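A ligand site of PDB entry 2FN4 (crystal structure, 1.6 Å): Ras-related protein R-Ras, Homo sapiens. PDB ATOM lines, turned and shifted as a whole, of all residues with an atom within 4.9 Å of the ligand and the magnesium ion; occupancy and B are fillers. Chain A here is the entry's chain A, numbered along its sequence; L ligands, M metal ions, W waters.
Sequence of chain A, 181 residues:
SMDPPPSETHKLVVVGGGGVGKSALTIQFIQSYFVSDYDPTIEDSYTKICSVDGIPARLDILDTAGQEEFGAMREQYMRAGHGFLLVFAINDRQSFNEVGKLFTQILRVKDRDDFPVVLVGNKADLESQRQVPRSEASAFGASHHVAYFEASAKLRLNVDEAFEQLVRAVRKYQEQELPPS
Merely in contact with the magnesium ion: Asp 63 (3.9 Å). Within 4 Å of the magnesium ion: Ser 23 and Asp 63. The nearest printed residue that does not touch the magnesium ion is Tyr 38 (4.4 Å).
Water W3 lies within hydrogen-bond range of O of Tyr 38, O5 of the ligand and O of Asp 39. Water W9 bridges O3 of the ligand and O of Pro 40. Water W8 bridges OD1 of Asp 63 (2.7 Å) and O of Thr 64 (2.9 Å). Water W2 lies within hydrogen-bond range of an oxygen (O5) of the ligand (2.6 Å) and the backbone carbonyl oxygen of Tyr 38 (3.1 Å). Water W6 lies within hydrogen-bond range of the backbone carbonyl oxygen of Val 35 (2.5 Å), an oxygen (O6) of the ligand (3.0 Å) and the backbone NH of Tyr 38 (3.1 Å). Water W5 lies within hydrogen-bond range of the side-chain amino group (NZ) of Lys 123 (2.9 Å) and a nitrogen (N5) of the ligand (3.1 Å).
The backbone NH (N) of Ser 23 sits at hydrogen-bond distance from the side-chain carboxylate (OD1) of Asp 63 (3.4 Å). NZ of Lys 22 is in hydrogen-bond range of O of Gly 17 (2.7 Å). OD1 of Asp 125 sits at hydrogen-bond distance from OG of Ser 152 (2.8 Å). N of Ala 153 is in hydrogen-bond range of OD1 of Asn 122. The side-chain amino group (NZ) of Lys 123 lies within hydrogen-bond range of the backbone carbonyl oxygen (O) of Gly 19. The side-chain hydroxyl of Ser 152 lies close to the backbone NH of Lys 154 (3.4 Å). The side-chain amide nitrogen of Asn 122 lies within hydrogen-bond range of the backbone carbonyl oxygen of Val 20.
The magnesium ion is bound by water W8, O2 of the ligand, water W9, OG of Ser 23, water W4 and water W3.
N of Ser 23 sits close to O6 of the ligand (3.5 Å). The backbone NH (N) of Lys 22 is in hydrogen-bond range of an oxygen (O1) of the ligand. An oxygen (O1) of the ligand lies within salt-bridge range of the side-chain amino group (NZ) of Lys 22 (2.6 Å). The backbone carbonyl oxygen (O) of Ser 36 lies within hydrogen-bond range of an oxygen (O10) of the ligand (2.6 Å). A nitrogen (N3) of the ligand lies within hydrogen-bond range of the side-chain carboxylate (OD1) of Asp 125 (2.8 Å). The backbone NH (N) of Ala 24 sits at hydrogen-bond distance from an oxygen (O6) of the ligand (2.8 Å). N of Ala 153 is in hydrogen-bond range of O11 of the ligand, 2.9 Å away. The backbone NH of Gly 19 is in hydrogen-bond range of an oxygen (O3) of the ligand (3.0 Å). The backbone NH of Lys 154 lies within hydrogen-bond range of an oxygen (O11) of the ligand (3.0 Å). The side-chain amino group (NZ) of Lys 123 lies within hydrogen-bond range of an oxygen (O8) of the ligand, 3.1 Å away. O4 of the ligand lies within hydrogen-bond range of N of Gly 21, 3.1 Å away. N2 of the ligand sits at hydrogen-bond distance from ND2 of Asn 122, at 3.2 Å. N of Val 20 sits at hydrogen-bond distance from O1 of the ligand, 3.5 Å away.
Merely in contact with the ligand: Ser 152, Leu 126, Tyr 38, Phe 34 and Gly 17. Hydrophobic or aromatic side chains within 4 Å of the ligand: Val 20, Ala 24, Phe 34, Leu 126 and Ala 153. Of the 25 residues printed, 17 come within 4 Å of the ligand. The nearest printed residue that does not touch the ligand is Gly 18 (4.0002 Å).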
ATOM      1  N   GLY A  17     -27.879 -20.659 -25.712  1.00  0.00           N
ATOM      2  CA  GLY A  17     -27.938 -20.775 -27.150  1.00  0.00           C
ATOM      3  C   GLY A  17     -26.910 -19.919 -27.837  1.00  0.00           C
ATOM      4  O   GLY A  17     -26.331 -19.016 -27.246  1.00  0.00           O
ATOM      5  N   GLY A  18     -26.673 -20.199 -29.119  1.00  0.00           N
ATOM      6  CA  GLY A  18     -25.709 -19.406 -29.864  1.00  0.00           C
ATOM      7  C   GLY A  18     -26.221 -17.994 -30.016  1.00  0.00           C
ATOM      8  O   GLY A  18     -27.428 -17.780 -30.148  1.00  0.00           O
ATOM      9  N   GLY A  19     -25.293 -17.047 -29.999  1.00  0.00           N
ATOM     10  CA  GLY A  19     -25.608 -15.657 -30.281  1.00  0.00           C
ATOM     11  C   GLY A  19     -26.229 -14.869 -29.147  1.00  0.00           C
ATOM     12  O   GLY A  19     -26.662 -13.743 -29.346  1.00  0.00           O
ATOM     13  N   VAL A  20     -26.298 -15.465 -27.960  1.00  0.00           N
ATOM     14  CA  VAL A  20     -26.908 -14.794 -26.789  1.00  0.00           C
ATOM     15  C   VAL A  20     -25.959 -13.861 -26.086  1.00  0.00           C
ATOM     16  O   VAL A  20     -26.403 -12.983 -25.383  1.00  0.00           O
ATOM     17  CB  VAL A  20     -27.471 -15.793 -25.762  1.00  0.00           C
ATOM     18  CG1 VAL A  20     -28.560 -16.610 -26.354  1.00  0.00           C
ATOM     19  CG2 VAL A  20     -26.382 -16.657 -25.115  1.00  0.00           C
ATOM     20  N   GLY A  21     -24.658 -14.065 -26.267  1.00  0.00           N
ATOM     21  CA  GLY A  21     -23.664 -13.222 -25.597  1.00  0.00           C
ATOM     22  C   GLY A  21     -22.755 -13.913 -24.586  1.00  0.00           C
ATOM     23  O   GLY A  21     -22.187 -13.247 -23.705  1.00  0.00           O
ATOM     24  N   LYS A  22     -22.660 -15.238 -24.633  1.00  0.00           N
ATOM     25  CA  LYS A  22     -21.757 -15.963 -23.731  1.00  0.00           C
ATOM     26  C   LYS A  22     -20.311 -15.481 -23.809  1.00  0.00           C
ATOM     27  O   LYS A  22     -19.695 -15.211 -22.790  1.00  0.00           O
ATOM     28  CB  LYS A  22     -21.807 -17.491 -23.929  1.00  0.00           C
ATOM     29  CG  LYS A  22     -23.202 -18.075 -23.866  1.00  0.00           C
ATOM     30  CD  LYS A  22     -23.297 -19.563 -24.096  1.00  0.00           C
ATOM     31  CE  LYS A  22     -22.922 -19.967 -25.518  1.00  0.00           C
ATOM     32  NZ  LYS A  22     -23.696 -19.305 -26.600  1.00  0.00           N
ATOM     33  N   SER A  23     -19.736 -15.394 -25.016  1.00  0.00           N
ATOM     34  CA  SER A  23     -18.360 -14.897 -25.140  1.00  0.00           C
ATOM     35  C   SER A  23     -18.208 -13.426 -24.714  1.00  0.00           C
ATOM     36  O   SER A  23     -17.237 -13.052 -24.050  1.00  0.00           O
ATOM     37  CB  SER A  23     -17.848 -15.063 -26.562  1.00  0.00           C
ATOM     38  OG  SER A  23     -17.903 -16.402 -26.923  1.00  0.00           O
ATOM     39  N   ALA A  24     -19.143 -12.604 -25.156  1.00  0.00           N
ATOM     40  CA  ALA A  24     -19.109 -11.195 -24.874  1.00  0.00           C
ATOM     41  C   ALA A  24     -19.192 -10.986 -23.355  1.00  0.00           C
ATOM     42  O   ALA A  24     -18.508 -10.125 -22.830  1.00  0.00           O
ATOM     43  CB  ALA A  24     -20.261 -10.478 -25.591  1.00  0.00           C
ATOM     44  N   PHE A  34     -15.623  -4.913 -24.520  1.00  0.00           N
ATOM     45  CA  PHE A  34     -16.640  -5.572 -25.329  1.00  0.00           C
ATOM     46  C   PHE A  34     -16.058  -6.066 -26.636  1.00  0.00           C
ATOM     47  O   PHE A  34     -15.508  -5.288 -27.444  1.00  0.00           O
ATOM     48  CB  PHE A  34     -17.791  -4.603 -25.605  1.00  0.00           C
ATOM     49  CG  PHE A  34     -18.931  -5.207 -26.395  1.00  0.00           C
ATOM     50  CD1 PHE A  34     -19.530  -6.385 -25.992  1.00  0.00           C
ATOM     51  CD2 PHE A  34     -19.439  -4.544 -27.499  1.00  0.00           C
ATOM     52  CE1 PHE A  34     -20.610  -6.911 -26.692  1.00  0.00           C
ATOM     53  CE2 PHE A  34     -20.520  -5.079 -28.225  1.00  0.00           C
ATOM     54  CZ  PHE A  34     -21.096  -6.251 -27.825  1.00  0.00           C
ATOM     55  N   VAL A  35     -16.181  -7.365 -26.858  1.00  0.00           N
ATOM     56  CA  VAL A  35     -15.850  -7.964 -28.170  1.00  0.00           C
ATOM     57  C   VAL A  35     -17.177  -8.293 -28.859  1.00  0.00           C
ATOM     58  O   VAL A  35     -17.947  -9.114 -28.345  1.00  0.00           O
ATOM     59  CB  VAL A  35     -14.997  -9.221 -28.003  1.00  0.00           C
ATOM     60  CG1 VAL A  35     -14.805  -9.914 -29.338  1.00  0.00           C
ATOM     61  CG2 VAL A  35     -13.642  -8.881 -27.371  1.00  0.00           C
ATOM     62  N   SER A  36     -17.455  -7.642 -29.986  1.00  0.00           N
ATOM     63  CA  SER A  36     -18.792  -7.696 -30.606  1.00  0.00           C
ATOM     64  C   SER A  36     -18.894  -8.814 -31.628  1.00  0.00           C
ATOM     65  O   SER A  36     -19.994  -9.120 -32.099  1.00  0.00           O
ATOM     66  CB  SER A  36     -19.156  -6.354 -31.248  1.00  0.00           C
ATOM     67  OG  SER A  36     -18.452  -6.145 -32.456  1.00  0.00           O
ATOM     68  N   ASP A  37     -17.769  -9.446 -31.947  1.00  0.00           N
ATOM     69  CA  ASP A  37     -17.715 -10.423 -33.037  1.00  0.00           C
ATOM     70  C   ASP A  37     -16.770 -11.577 -32.706  1.00  0.00           C
ATOM     71  O   ASP A  37     -15.910 -11.951 -33.523  1.00  0.00           O
ATOM     72  CB  ASP A  37     -17.319  -9.726 -34.354  1.00  0.00           C
ATOM     73  CG  ASP A  37     -16.009  -8.918 -34.253  1.00  0.00           C
ATOM     74  OD1 ASP A  37     -15.318  -8.947 -33.218  1.00  0.00           O
ATOM     75  OD2 ASP A  37     -15.663  -8.257 -35.259  1.00  0.00           O
ATOM     76  N   TYR A  38     -16.948 -12.161 -31.511  1.00  0.00           N
ATOM     77  CA  TYR A  38     -16.084 -13.257 -31.090  1.00  0.00           C
ATOM     78  C   TYR A  38     -16.397 -14.539 -31.857  1.00  0.00           C
ATOM     79  O   TYR A  38     -17.498 -15.072 -31.759  1.00  0.00           O
ATOM     80  CB  TYR A  38     -16.135 -13.539 -29.588  1.00  0.00           C
ATOM     81  CG  TYR A  38     -14.999 -14.476 -29.150  1.00  0.00           C
ATOM     82  CD1 TYR A  38     -13.685 -14.032 -29.113  1.00  0.00           C
ATOM     83  CD2 TYR A  38     -15.246 -15.801 -28.823  1.00  0.00           C
ATOM     84  CE1 TYR A  38     -12.644 -14.880 -28.721  1.00  0.00           C
ATOM     85  CE2 TYR A  38     -14.222 -16.648 -28.431  1.00  0.00           C
ATOM     86  CZ  TYR A  38     -12.912 -16.183 -28.385  1.00  0.00           C
ATOM     87  OH  TYR A  38     -11.871 -17.026 -28.016  1.00  0.00           O
ATOM     88  N   ASP A  39     -15.408 -15.001 -32.616  1.00  0.00           N
ATOM     89  CA  ASP A  39     -15.423 -16.330 -33.198  1.00  0.00           C
ATOM     90  C   ASP A  39     -16.435 -17.229 -32.484  1.00  0.00           C
ATOM     91  O   ASP A  39     -16.184 -17.678 -31.345  1.00  0.00           O
ATOM     92  CB  ASP A  39     -14.017 -16.928 -33.104  1.00  0.00           C
ATOM     93  CG  ASP A  39     -13.837 -18.120 -34.014  1.00  0.00           C
ATOM     94  OD1 ASP A  39     -12.662 -18.390 -34.412  1.00  0.00           O
ATOM     95  OD2 ASP A  39     -14.838 -18.782 -34.347  1.00  0.00           O
ATOM     96  N   PRO A  40     -17.609 -17.451 -33.118  1.00  0.00           N
ATOM     97  CA  PRO A  40     -18.622 -18.315 -32.496  1.00  0.00           C
ATOM     98  C   PRO A  40     -18.192 -19.750 -32.340  1.00  0.00           C
ATOM     99  O   PRO A  40     -18.767 -20.463 -31.521  1.00  0.00           O
ATOM    100  CB  PRO A  40     -19.832 -18.212 -33.439  1.00  0.00           C
ATOM    101  CG  PRO A  40     -19.396 -17.493 -34.639  1.00  0.00           C
ATOM    102  CD  PRO A  40     -18.073 -16.838 -34.371  1.00  0.00           C
ATOM    103  N   ILE A  42     -15.180 -20.708 -31.250  1.00  0.00           N
ATOM    104  CA  ILE A  42     -14.140 -20.886 -30.237  1.00  0.00           C
ATOM    105  C   ILE A  42     -14.769 -21.170 -28.875  1.00  0.00           C
ATOM    106  O   ILE A  42     -15.565 -20.378 -28.364  1.00  0.00           O
ATOM    107  CB  ILE A  42     -13.187 -19.675 -30.141  1.00  0.00           C
ATOM    108  CG1 ILE A  42     -12.268 -19.637 -31.366  1.00  0.00           C
ATOM    109  CG2 ILE A  42     -12.326 -19.770 -28.894  1.00  0.00           C
ATOM    110  CD1 ILE A  42     -11.485 -18.347 -31.480  1.00  0.00           C
ATOM    111  N   ASP A  63     -16.261 -20.896 -21.484  1.00  0.00           N
ATOM    112  CA  ASP A  63     -17.205 -20.265 -22.406  1.00  0.00           C
ATOM    113  C   ASP A  63     -17.529 -21.260 -23.523  1.00  0.00           C
ATOM    114  O   ASP A  63     -16.746 -21.422 -24.455  1.00  0.00           O
ATOM    115  CB  ASP A  63     -16.554 -19.006 -22.993  1.00  0.00           C
ATOM    116  CG  ASP A  63     -17.361 -18.389 -24.126  1.00  0.00           C
ATOM    117  OD1 ASP A  63     -18.613 -18.506 -24.122  1.00  0.00           O
ATOM    118  OD2 ASP A  63     -16.715 -17.798 -25.007  1.00  0.00           O
ATOM    119  N   THR A  64     -18.689 -21.904 -23.423  1.00  0.00           N
ATOM    120  CA  THR A  64     -19.030 -23.005 -24.350  1.00  0.00           C
ATOM    121  C   THR A  64     -19.436 -22.504 -25.742  1.00  0.00           C
ATOM    122  O   THR A  64     -20.076 -21.470 -25.887  1.00  0.00           O
ATOM    123  CB  THR A  64     -20.147 -23.923 -23.780  1.00  0.00           C
ATOM    124  OG1 THR A  64     -21.348 -23.178 -23.553  1.00  0.00           O
ATOM    125  CG2 THR A  64     -19.694 -24.570 -22.464  1.00  0.00           C
ATOM    126  N   ASN A 122     -29.318 -11.461 -21.207  1.00  0.00           N
ATOM    127  CA  ASN A 122     -28.412 -10.482 -21.793  1.00  0.00           C
ATOM    128  C   ASN A 122     -29.083  -9.572 -22.847  1.00  0.00           C
ATOM    129  O   ASN A 122     -30.223  -9.814 -23.269  1.00  0.00           O
ATOM    130  CB  ASN A 122     -27.200 -11.238 -22.403  1.00  0.00           C
ATOM    131  CG  ASN A 122     -26.073 -10.317 -22.826  1.00  0.00           C
ATOM    132  OD1 ASN A 122     -25.725  -9.360 -22.136  1.00  0.00           O
ATOM    133  ND2 ASN A 122     -25.476 -10.634 -23.982  1.00  0.00           N
ATOM    134  N   LYS A 123     -28.342  -8.540 -23.256  1.00  0.00           N
ATOM    135  CA  LYS A 123     -28.769  -7.548 -24.267  1.00  0.00           C
ATOM    136  C   LYS A 123     -29.845  -6.625 -23.701  1.00  0.00           C
ATOM    137  O   LYS A 123     -30.790  -6.229 -24.379  1.00  0.00           O
ATOM    138  CB  LYS A 123     -29.187  -8.197 -25.577  1.00  0.00           C
ATOM    139  CG  LYS A 123     -28.215  -9.251 -26.074  1.00  0.00           C
ATOM    140  CD  LYS A 123     -28.385  -9.565 -27.533  1.00  0.00           C
ATOM    141  CE  LYS A 123     -27.491 -10.689 -27.951  1.00  0.00           C
ATOM    142  NZ  LYS A 123     -27.549 -11.084 -29.375  1.00  0.00           N
ATOM    143  N   ASP A 125     -29.602  -3.638 -23.239  1.00  0.00           N
ATOM    144  CA  ASP A 125     -29.559  -2.403 -23.987  1.00  0.00           C
ATOM    145  C   ASP A 125     -30.561  -2.352 -25.191  1.00  0.00           C
ATOM    146  O   ASP A 125     -30.701  -1.307 -25.841  1.00  0.00           O
ATOM    147  CB  ASP A 125     -28.114  -2.177 -24.481  1.00  0.00           C
ATOM    148  CG  ASP A 125     -27.618  -3.340 -25.328  1.00  0.00           C
ATOM    149  OD1 ASP A 125     -27.317  -4.386 -24.724  1.00  0.00           O
ATOM    150  OD2 ASP A 125     -27.574  -3.215 -26.572  1.00  0.00           O
ATOM    151  N   LEU A 126     -31.219  -3.480 -25.462  1.00  0.00           N
ATOM    152  CA  LEU A 126     -32.178  -3.623 -26.585  1.00  0.00           C
ATOM    153  C   LEU A 126     -33.616  -3.753 -26.032  1.00  0.00           C
ATOM    154  O   LEU A 126     -34.411  -4.587 -26.478  1.00  0.00           O
ATOM    155  CB  LEU A 126     -31.831  -4.883 -27.371  1.00  0.00           C
ATOM    156  CG  LEU A 126     -30.429  -4.924 -27.994  1.00  0.00           C
ATOM    157  CD1 LEU A 126     -30.292  -6.206 -28.807  1.00  0.00           C
ATOM    158  CD2 LEU A 126     -30.153  -3.690 -28.843  1.00  0.00           C
ATOM    159  N   SER A 152     -26.047  -6.466 -19.782  1.00  0.00           N
ATOM    160  CA  SER A 152     -25.634  -6.034 -21.120  1.00  0.00           C
ATOM    161  C   SER A 152     -24.124  -6.202 -21.167  1.00  0.00           C
ATOM    162  O   SER A 152     -23.391  -5.465 -20.494  1.00  0.00           O
ATOM    163  CB  SER A 152     -25.991  -4.569 -21.401  1.00  0.00           C
ATOM    164  OG  SER A 152     -25.479  -4.082 -22.657  1.00  0.00           O
ATOM    165  N   ALA A 153     -23.654  -7.168 -21.940  1.00  0.00           N
ATOM    166  CA  ALA A 153     -22.227  -7.290 -22.168  1.00  0.00           C
ATOM    167  C   ALA A 153     -21.721  -6.041 -22.930  1.00  0.00           C
ATOM    168  O   ALA A 153     -20.612  -5.555 -22.687  1.00  0.00           O
ATOM    169  CB  ALA A 153     -21.932  -8.565 -22.931  1.00  0.00           C
ATOM    170  N   LYS A 154     -22.566  -5.505 -23.813  1.00  0.00           N
ATOM    171  CA  LYS A 154     -22.219  -4.348 -24.634  1.00  0.00           C
ATOM    172  C   LYS A 154     -21.866  -3.132 -23.774  1.00  0.00           C
ATOM    173  O   LYS A 154     -20.868  -2.401 -24.048  1.00  0.00           O
ATOM    174  CB  LYS A 154     -23.358  -4.023 -25.621  1.00  0.00           C
ATOM    175  CG  LYS A 154     -23.149  -2.721 -26.362  1.00  0.00           C
ATOM    176  CD  LYS A 154     -24.164  -2.483 -27.454  1.00  0.00           C
ATOM    177  CE  LYS A 154     -23.836  -1.202 -28.239  1.00  0.00           C
ATOM    178  NZ  LYS A 154     -24.734  -1.077 -29.412  1.00  0.00           N
HETATM  179  P1  LIG L   1     -22.151 -16.289 -28.040  1.00  0.00           P
HETATM  180  O1  LIG L   1     -23.212 -16.793 -27.091  1.00  0.00           O
HETATM  181  O2  LIG L   1     -20.748 -16.481 -27.576  1.00  0.00           O
HETATM  182  O3  LIG L   1     -22.395 -17.004 -29.397  1.00  0.00           O
HETATM  183  O4  LIG L   1     -22.432 -14.736 -28.315  1.00  0.00           O
HETATM  184  P2  LIG L   1     -21.430 -13.594 -28.712  1.00  0.00           P
HETATM  185  O5  LIG L   1     -20.587 -14.055 -29.887  1.00  0.00           O
HETATM  186  O6  LIG L   1     -20.549 -13.146 -27.562  1.00  0.00           O
HETATM  187  O7  LIG L   1     -22.492 -12.502 -29.151  1.00  0.00           O
HETATM  188  C1  LIG L   1     -23.355 -12.777 -30.266  1.00  0.00           C
HETATM  189  C2  LIG L   1     -23.840 -11.513 -30.915  1.00  0.00           C
HETATM  190  O8  LIG L   1     -24.560 -10.754 -29.945  1.00  0.00           O
HETATM  191  C3  LIG L   1     -22.735 -10.611 -31.443  1.00  0.00           C
HETATM  192  O9  LIG L   1     -23.197  -9.986 -32.655  1.00  0.00           O
HETATM  193  C4  LIG L   1     -22.566  -9.577 -30.352  1.00  0.00           C
HETATM  194  O10 LIG L   1     -22.113  -8.301 -30.823  1.00  0.00           O
HETATM  195  C5  LIG L   1     -23.989  -9.471 -29.822  1.00  0.00           C
HETATM  196  N1  LIG L   1     -24.077  -9.098 -28.384  1.00  0.00           N
HETATM  197  C6  LIG L   1     -23.484  -9.755 -27.368  1.00  0.00           C
HETATM  198  N2  LIG L   1     -23.773  -9.144 -26.188  1.00  0.00           N
HETATM  199  C7  LIG L   1     -24.592  -8.123 -26.483  1.00  0.00           C
HETATM  200  C8  LIG L   1     -25.237  -7.060 -25.731  1.00  0.00           C
HETATM  201  O11 LIG L   1     -25.104  -7.051 -24.494  1.00  0.00           O
HETATM  202  N3  LIG L   1     -25.999  -6.155 -26.371  1.00  0.00           N
HETATM  203  C9  LIG L   1     -26.130  -6.191 -27.719  1.00  0.00           C
HETATM  204  N4  LIG L   1     -26.901  -5.271 -28.296  1.00  0.00           N
HETATM  205  N5  LIG L   1     -25.566  -7.137 -28.481  1.00  0.00           N
HETATM  206  C10 LIG L   1     -24.774  -8.074 -27.937  1.00  0.00           C
HETATM  207 MG    MG M   1     -19.119 -17.652 -28.114  1.00  0.00          MG
HETATM  208  O   HOH W   1     -23.663  -6.069 -31.774  1.00  0.00           O
HETATM  209  O   HOH W   2     -20.025 -13.372 -32.321  1.00  0.00           O
HETATM  210  O   HOH W   3     -18.706 -16.025 -29.807  1.00  0.00           O
HETATM  211  O   HOH W   4     -17.439 -18.814 -28.843  1.00  0.00           O
HETATM  212  O   HOH W   5     -27.148  -8.520 -30.740  1.00  0.00           O
HETATM  213  O   HOH W   6     -18.609 -11.460 -29.048  1.00  0.00           O
HETATM  214  O   HOH W   7     -22.182 -16.047 -31.878  1.00  0.00           O
HETATM  215  O   HOH W   8     -19.103 -18.829 -26.726  1.00  0.00           O
HETATM  216  O   HOH W   9     -20.414 -18.777 -29.288  1.00  0.00           O
HETATM  217  O   HOH W  10     -26.698  -5.356 -31.413  1.00  0.00           O
